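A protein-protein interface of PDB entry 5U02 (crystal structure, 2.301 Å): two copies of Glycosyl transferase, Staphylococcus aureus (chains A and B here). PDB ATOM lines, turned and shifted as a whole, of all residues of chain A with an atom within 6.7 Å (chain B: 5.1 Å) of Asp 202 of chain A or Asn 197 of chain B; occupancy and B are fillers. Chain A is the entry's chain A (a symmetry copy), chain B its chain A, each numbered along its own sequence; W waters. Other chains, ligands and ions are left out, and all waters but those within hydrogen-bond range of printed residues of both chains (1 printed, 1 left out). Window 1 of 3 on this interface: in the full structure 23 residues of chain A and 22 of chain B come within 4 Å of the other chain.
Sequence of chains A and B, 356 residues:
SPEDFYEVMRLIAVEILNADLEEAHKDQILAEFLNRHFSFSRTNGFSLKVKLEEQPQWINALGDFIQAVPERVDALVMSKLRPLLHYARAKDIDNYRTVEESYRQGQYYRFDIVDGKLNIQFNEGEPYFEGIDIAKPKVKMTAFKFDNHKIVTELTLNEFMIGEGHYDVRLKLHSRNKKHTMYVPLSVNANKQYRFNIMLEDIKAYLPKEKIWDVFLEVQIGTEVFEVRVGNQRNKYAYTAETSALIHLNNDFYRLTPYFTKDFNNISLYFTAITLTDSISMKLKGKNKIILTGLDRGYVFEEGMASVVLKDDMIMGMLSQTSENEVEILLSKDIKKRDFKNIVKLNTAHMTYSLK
The side-chain carboxylate (OD2) of Asp 202 of chain A lies within hydrogen-bond range of the side-chain amide nitrogen (ND2) of Asn 197 of chain B (3.0 Å). NE of Arg 195 of chain B sits at hydrogen-bond distance from OH of Tyr 206 of chain A. NZ of Lys 150 of chain B is in salt-bridge range of OE2 of Glu 201 of chain A (2.6 Å).
N of Ser 187 of chain B sits at hydrogen-bond distance from O of Arg 195 of chain B, 3.0 Å away. The backbone carbonyl oxygen (O) of Val 188 of chain B sits at hydrogen-bond distance from the backbone NH (N) of Arg 195 of chain B, 3.0 Å away. OG of Ser 187 of chain B is in hydrogen-bond range of N of Asn 197 of chain B (3.0 Å).
Among the printed residues, pairs that only touch across the chains: Asp 202 of chain A with Val 188 of chain B, Ala 205 of chain A with Arg 195 of chain B and Asp 202 of chain A with Arg 195 of chain B.
Asp 202 of chain A touches three residues of chain B. Of chain A, only Asp 202 (3.0 Å) comes within 4 Å of Asn 197 of chain B. Of the printed residues of chain B, Tyr 206 of chain A touches Arg 195. Printed residues of chain B within 4 Å of Ala 205 of chain A: Arg 195. The nearest residue of chain B that does not touch Asp 202 of chain A is Ser 187 of chain B (4.7 Å). The nearest printed residue of chain B that does not touch Ala 205 of chain A is Val 188 of chain B (8.3 Å).
Of the 11 printed residues of chain B, 4 touch a printed residue of chain A. Of the 11 printed residues of chain A, 4 touch a printed residue of chain B. Printed residues of chain A that touch a printed residue of chain B: Glu 201, Asp 202, Ala 205 and Tyr 206. Among the printed residues, 6 pairs touch across the chains. Among the printed residues, Asp or Glu carboxylates within 4 Å of a Lys or Arg side-chain nitrogen of the other chain: Glu 201 of chain A with Lys 150 of chain B (2.6 Å).
Positions printed for both chains: 197, 198 and 199. Of the 6 pairs that touch across the chains among the printed residues, none has its exchanged pair printed and touching as well.
Water W1 lies within hydrogen-bond range of NH1 of Arg 195 of chain B (2.6 Å), OD2 of Asp 202 of chain A (3.1 Å) and OD1 of Asn 197 of chain B (3.1 Å).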
ATOM      1  N   MET A 182      17.919  18.167   3.555  1.00  0.00           N
ATOM      2  CA  MET A 182      16.768  17.312   3.310  1.00  0.00           C
ATOM      3  C   MET A 182      17.153  16.295   2.251  1.00  0.00           C
ATOM      4  O   MET A 182      17.820  16.641   1.274  1.00  0.00           O
ATOM      5  CB  MET A 182      15.529  18.100   2.847  1.00  0.00           C
ATOM      6  CG  MET A 182      14.894  18.987   3.916  1.00  0.00           C
ATOM      7  SD  MET A 182      13.285  19.631   3.396  1.00  0.00           S
ATOM      8  CE  MET A 182      13.638  21.380   3.267  1.00  0.00           C
ATOM      9  N   ASN A 197       9.590  12.439  -6.527  1.00  0.00           N
ATOM     10  CA  ASN A 197       8.380  13.135  -6.100  1.00  0.00           C
ATOM     11  C   ASN A 197       8.655  13.739  -4.730  1.00  0.00           C
ATOM     12  O   ASN A 197       8.812  13.006  -3.749  1.00  0.00           O
ATOM     13  CB  ASN A 197       7.182  12.190  -6.036  1.00  0.00           C
ATOM     14  CG  ASN A 197       6.860  11.553  -7.375  1.00  0.00           C
ATOM     15  OD1 ASN A 197       7.026  12.165  -8.425  1.00  0.00           O
ATOM     16  ND2 ASN A 197       6.396  10.310  -7.338  1.00  0.00           N
ATOM     17  N   ILE A 198       8.724  15.065  -4.666  1.00  0.00           N
ATOM     18  CA  ILE A 198       8.946  15.792  -3.420  1.00  0.00           C
ATOM     19  C   ILE A 198       7.590  16.299  -2.951  1.00  0.00           C
ATOM     20  O   ILE A 198       7.106  17.336  -3.418  1.00  0.00           O
ATOM     21  CB  ILE A 198       9.927  16.952  -3.599  1.00  0.00           C
ATOM     22  CG1 ILE A 198      11.255  16.473  -4.179  1.00  0.00           C
ATOM     23  CG2 ILE A 198      10.152  17.658  -2.279  1.00  0.00           C
ATOM     24  CD1 ILE A 198      12.076  17.613  -4.705  1.00  0.00           C
ATOM     25  N   MET A 199       6.982  15.577  -2.017  1.00  0.00           N
ATOM     26  CA  MET A 199       5.682  15.950  -1.476  1.00  0.00           C
ATOM     27  C   MET A 199       5.853  17.100  -0.488  1.00  0.00           C
ATOM     28  O   MET A 199       6.553  16.960   0.520  1.00  0.00           O
ATOM     29  CB  MET A 199       5.039  14.742  -0.800  1.00  0.00           C
ATOM     30  CG  MET A 199       5.188  13.463  -1.600  1.00  0.00           C
ATOM     31  SD  MET A 199       4.536  13.643  -3.263  1.00  0.00           S
ATOM     32  CE  MET A 199       2.788  13.729  -2.912  1.00  0.00           C
ATOM     33  N   LEU A 200       5.201  18.231  -0.766  1.00  0.00           N
ATOM     34  CA  LEU A 200       5.371  19.407   0.082  1.00  0.00           C
ATOM     35  C   LEU A 200       4.850  19.177   1.496  1.00  0.00           C
ATOM     36  O   LEU A 200       5.342  19.809   2.438  1.00  0.00           O
ATOM     37  CB  LEU A 200       4.683  20.617  -0.546  1.00  0.00           C
ATOM     38  CG  LEU A 200       5.046  20.897  -2.003  1.00  0.00           C
ATOM     39  CD1 LEU A 200       4.249  22.052  -2.541  1.00  0.00           C
ATOM     40  CD2 LEU A 200       6.517  21.184  -2.146  1.00  0.00           C
ATOM     41  N   GLU A 201       3.866  18.289   1.670  1.00  0.00           N
ATOM     42  CA  GLU A 201       3.451  17.918   3.021  1.00  0.00           C
ATOM     43  C   GLU A 201       4.589  17.247   3.783  1.00  0.00           C
ATOM     44  O   GLU A 201       4.663  17.359   5.012  1.00  0.00           O
ATOM     45  CB  GLU A 201       2.224  17.003   2.964  1.00  0.00           C
ATOM     46  CG  GLU A 201       1.690  16.552   4.329  1.00  0.00           C
ATOM     47  CD  GLU A 201       0.532  15.563   4.213  1.00  0.00           C
ATOM     48  OE1 GLU A 201       0.019  15.367   3.091  1.00  0.00           O
ATOM     49  OE2 GLU A 201       0.139  14.974   5.243  1.00  0.00           O
ATOM     50  N   ASP A 202       5.496  16.564   3.075  1.00  0.00           N
ATOM     51  CA  ASP A 202       6.627  15.925   3.738  1.00  0.00           C
ATOM     52  C   ASP A 202       7.711  16.924   4.138  1.00  0.00           C
ATOM     53  O   ASP A 202       8.401  16.708   5.143  1.00  0.00           O
ATOM     54  CB  ASP A 202       7.234  14.838   2.839  1.00  0.00           C
ATOM     55  CG  ASP A 202       6.321  13.632   2.664  1.00  0.00           C
ATOM     56  OD1 ASP A 202       6.535  12.873   1.698  1.00  0.00           O
ATOM     57  OD2 ASP A 202       5.394  13.448   3.482  1.00  0.00           O
ATOM     58  N   ILE A 203       7.881  18.011   3.385  1.00  0.00           N
ATOM     59  CA  ILE A 203       8.973  18.955   3.610  1.00  0.00           C
ATOM     60  C   ILE A 203       8.504  20.275   4.203  1.00  0.00           C
ATOM     61  O   ILE A 203       9.347  21.136   4.500  1.00  0.00           O
ATOM     62  CB  ILE A 203       9.769  19.208   2.315  1.00  0.00           C
ATOM     63  CG1 ILE A 203       8.956  20.036   1.320  1.00  0.00           C
ATOM     64  CG2 ILE A 203      10.185  17.895   1.671  1.00  0.00           C
ATOM     65  CD1 ILE A 203       9.741  20.381   0.063  1.00  0.00           C
ATOM     66  N   LYS A 204       7.195  20.464   4.394  1.00  0.00           N
ATOM     67  CA  LYS A 204       6.683  21.718   4.945  1.00  0.00           C
ATOM     68  C   LYS A 204       7.273  22.023   6.318  1.00  0.00           C
ATOM     69  O   LYS A 204       7.573  23.182   6.627  1.00  0.00           O
ATOM     70  CB  LYS A 204       5.157  21.665   5.049  1.00  0.00           C
ATOM     71  CG  LYS A 204       4.429  22.403   3.958  1.00  0.00           C
ATOM     72  CD  LYS A 204       3.082  22.929   4.444  1.00  0.00           C
ATOM     73  CE  LYS A 204       2.258  21.867   5.135  1.00  0.00           C
ATOM     74  NZ  LYS A 204       0.851  22.323   5.309  1.00  0.00           N
ATOM     75  N   ALA A 205       7.425  21.003   7.161  1.00  0.00           N
ATOM     76  CA  ALA A 205       7.888  21.240   8.522  1.00  0.00           C
ATOM     77  C   ALA A 205       9.351  21.658   8.578  1.00  0.00           C
ATOM     78  O   ALA A 205       9.758  22.303   9.549  1.00  0.00           O
ATOM     79  CB  ALA A 205       7.676  19.985   9.374  1.00  0.00           C
ATOM     80  N   TYR A 206      10.143  21.317   7.560  1.00  0.00           N
ATOM     81  CA  TYR A 206      11.578  21.568   7.577  1.00  0.00           C
ATOM     82  C   TYR A 206      11.991  22.798   6.778  1.00  0.00           C
ATOM     83  O   TYR A 206      13.036  23.386   7.077  1.00  0.00           O
ATOM     84  CB  TYR A 206      12.324  20.334   7.049  1.00  0.00           C
ATOM     85  CG  TYR A 206      11.888  19.050   7.722  1.00  0.00           C
ATOM     86  CD1 TYR A 206      12.030  18.883   9.094  1.00  0.00           C
ATOM     87  CD2 TYR A 206      11.342  18.007   6.991  1.00  0.00           C
ATOM     88  CE1 TYR A 206      11.636  17.715   9.720  1.00  0.00           C
ATOM     89  CE2 TYR A 206      10.943  16.827   7.607  1.00  0.00           C
ATOM     90  CZ  TYR A 206      11.090  16.691   8.973  1.00  0.00           C
ATOM     91  OH  TYR A 206      10.699  15.530   9.598  1.00  0.00           O
ATOM     92  N   LYS B 150      -3.401   7.476   7.366  1.00  0.00           N
ATOM     93  CA  LYS B 150      -1.980   7.204   7.518  1.00  0.00           C
ATOM     94  C   LYS B 150      -1.516   7.576   8.918  1.00  0.00           C
ATOM     95  O   LYS B 150      -2.183   8.315   9.646  1.00  0.00           O
ATOM     96  CB  LYS B 150      -1.146   7.964   6.482  1.00  0.00           C
ATOM     97  CG  LYS B 150      -1.238   9.472   6.620  1.00  0.00           C
ATOM     98  CD  LYS B 150      -0.293  10.182   5.658  1.00  0.00           C
ATOM     99  CE  LYS B 150      -0.408  11.690   5.807  1.00  0.00           C
ATOM    100  NZ  LYS B 150       0.525  12.405   4.899  1.00  0.00           N
ATOM    101  N   ILE B 151      -0.346   7.052   9.272  1.00  0.00           N
ATOM    102  CA  ILE B 151       0.394   7.450  10.461  1.00  0.00           C
ATOM    103  C   ILE B 151       1.645   8.183  10.002  1.00  0.00           C
ATOM    104  O   ILE B 151       2.358   7.705   9.111  1.00  0.00           O
ATOM    105  CB  ILE B 151       0.765   6.234  11.327  1.00  0.00           C
ATOM    106  CG1 ILE B 151      -0.488   5.492  11.795  1.00  0.00           C
ATOM    107  CG2 ILE B 151       1.638   6.652  12.507  1.00  0.00           C
ATOM    108  CD1 ILE B 151      -0.192   4.090  12.316  1.00  0.00           C
ATOM    109  N   VAL B 152       1.911   9.339  10.600  1.00  0.00           N
ATOM    110  CA  VAL B 152       3.126  10.103  10.338  1.00  0.00           C
ATOM    111  C   VAL B 152       3.893  10.206  11.646  1.00  0.00           C
ATOM    112  O   VAL B 152       3.395  10.790  12.620  1.00  0.00           O
ATOM    113  CB  VAL B 152       2.819  11.497   9.772  1.00  0.00           C
ATOM    114  CG1 VAL B 152       4.114  12.241   9.435  1.00  0.00           C
ATOM    115  CG2 VAL B 152       1.924  11.382   8.552  1.00  0.00           C
ATOM    116  N   VAL B 184       8.654  -0.352   7.191  1.00  0.00           N
ATOM    117  CA  VAL B 184       8.190   0.824   6.461  1.00  0.00           C
ATOM    118  C   VAL B 184       9.413   1.623   6.025  1.00  0.00           C
ATOM    119  O   VAL B 184      10.232   2.002   6.872  1.00  0.00           O
ATOM    120  CB  VAL B 184       7.253   1.690   7.315  1.00  0.00           C
ATOM    121  CG1 VAL B 184       6.706   2.835   6.482  1.00  0.00           C
ATOM    122  CG2 VAL B 184       6.132   0.849   7.892  1.00  0.00           C
ATOM    123  N   SER B 187      10.451   8.011   4.455  1.00  0.00           N
ATOM    124  CA  SER B 187       9.770   8.885   3.502  1.00  0.00           C
ATOM    125  C   SER B 187      10.596  10.119   3.168  1.00  0.00           C
ATOM    126  O   SER B 187      10.626  10.548   2.012  1.00  0.00           O
ATOM    127  CB  SER B 187       8.411   9.318   4.053  1.00  0.00           C
ATOM    128  OG  SER B 187       7.547   8.202   4.213  1.00  0.00           O
ATOM    129  N   VAL B 188      11.268  10.690   4.167  1.00  0.00           N
ATOM    130  CA  VAL B 188      12.131  11.855   4.006  1.00  0.00           C
ATOM    131  C   VAL B 188      12.917  12.005   5.300  1.00  0.00           C
ATOM    132  O   VAL B 188      12.451  11.597   6.369  1.00  0.00           O
ATOM    133  CB  VAL B 188      11.313  13.128   3.696  1.00  0.00           C
ATOM    134  CG1 VAL B 188      10.460  13.531   4.901  1.00  0.00           C
ATOM    135  CG2 VAL B 188      12.218  14.275   3.277  1.00  0.00           C
ATOM    136  N   ARG B 195      11.401  10.793   9.013  1.00  0.00           N
ATOM    137  CA  ARG B 195       9.945  10.831   8.936  1.00  0.00           C
ATOM    138  C   ARG B 195       9.422   9.639   8.147  1.00  0.00           C
ATOM    139  O   ARG B 195       9.887   9.373   7.034  1.00  0.00           O
ATOM    140  CB  ARG B 195       9.472  12.132   8.287  1.00  0.00           C
ATOM    141  CG  ARG B 195       7.995  12.151   7.922  1.00  0.00           C
ATOM    142  CD  ARG B 195       7.619  13.504   7.358  1.00  0.00           C
ATOM    143  NE  ARG B 195       7.786  14.547   8.361  1.00  0.00           N
ATOM    144  CZ  ARG B 195       6.796  15.299   8.823  1.00  0.00           C
ATOM    145  NH1 ARG B 195       5.568  15.144   8.346  1.00  0.00           N
ATOM    146  NH2 ARG B 195       7.043  16.220   9.744  1.00  0.00           N
ATOM    147  N   PHE B 196       8.441   8.943   8.713  1.00  0.00           N
ATOM    148  CA  PHE B 196       7.851   7.763   8.096  1.00  0.00           C
ATOM    149  C   PHE B 196       6.357   7.992   7.914  1.00  0.00           C
ATOM    150  O   PHE B 196       5.653   8.314   8.879  1.00  0.00           O
ATOM    151  CB  PHE B 196       8.104   6.513   8.943  1.00  0.00           C
ATOM    152  CG  PHE B 196       9.559   6.160   9.092  1.00  0.00           C
ATOM    153  CD1 PHE B 196      10.342   6.754  10.077  1.00  0.00           C
ATOM    154  CD2 PHE B 196      10.147   5.250   8.229  1.00  0.00           C
ATOM    155  CE1 PHE B 196      11.689   6.426  10.207  1.00  0.00           C
ATOM    156  CE2 PHE B 196      11.481   4.921   8.346  1.00  0.00           C
ATOM    157  CZ  PHE B 196      12.256   5.507   9.336  1.00  0.00           C
ATOM    158  N   ASN B 197       5.882   7.845   6.672  1.00  0.00           N
ATOM    159  CA  ASN B 197       4.456   7.814   6.360  1.00  0.00           C
ATOM    160  C   ASN B 197       4.035   6.353   6.277  1.00  0.00           C
ATOM    161  O   ASN B 197       4.450   5.639   5.359  1.00  0.00           O
ATOM    162  CB  ASN B 197       4.154   8.532   5.045  1.00  0.00           C
ATOM    163  CG  ASN B 197       4.555   9.995   5.065  1.00  0.00           C
ATOM    164  OD1 ASN B 197       4.472  10.662   6.092  1.00  0.00           O
ATOM    165  ND2 ASN B 197       4.997  10.499   3.920  1.00  0.00           N
ATOM    166  N   ILE B 198       3.227   5.911   7.236  1.00  0.00           N
ATOM    167  CA  ILE B 198       2.710   4.547   7.274  1.00  0.00           C
ATOM    168  C   ILE B 198       1.288   4.593   6.732  1.00  0.00           C
ATOM    169  O   ILE B 198       0.344   4.923   7.457  1.00  0.00           O
ATOM    170  CB  ILE B 198       2.733   3.964   8.688  1.00  0.00           C
ATOM    171  CG1 ILE B 198       4.134   4.018   9.289  1.00  0.00           C
ATOM    172  CG2 ILE B 198       2.218   2.540   8.677  1.00  0.00           C
ATOM    173  CD1 ILE B 198       4.111   3.809  10.774  1.00  0.00           C
ATOM    174  N   MET B 199       1.132   4.246   5.459  1.00  0.00           N
ATOM    175  CA  MET B 199      -0.174   4.242   4.814  1.00  0.00           C
ATOM    176  C   MET B 199      -0.956   3.009   5.254  1.00  0.00           C
ATOM    177  O   MET B 199      -0.519   1.877   5.024  1.00  0.00           O
ATOM    178  CB  MET B 199       0.000   4.265   3.298  1.00  0.00           C
ATOM    179  CG  MET B 199       1.070   5.234   2.835  1.00  0.00           C
ATOM    180  SD  MET B 199       0.758   6.898   3.433  1.00  0.00           S
ATOM    181  CE  MET B 199      -0.666   7.328   2.447  1.00  0.00           C
HETATM  182  O   HOH W   1       4.420  13.774   6.396  1.00  0.00           O
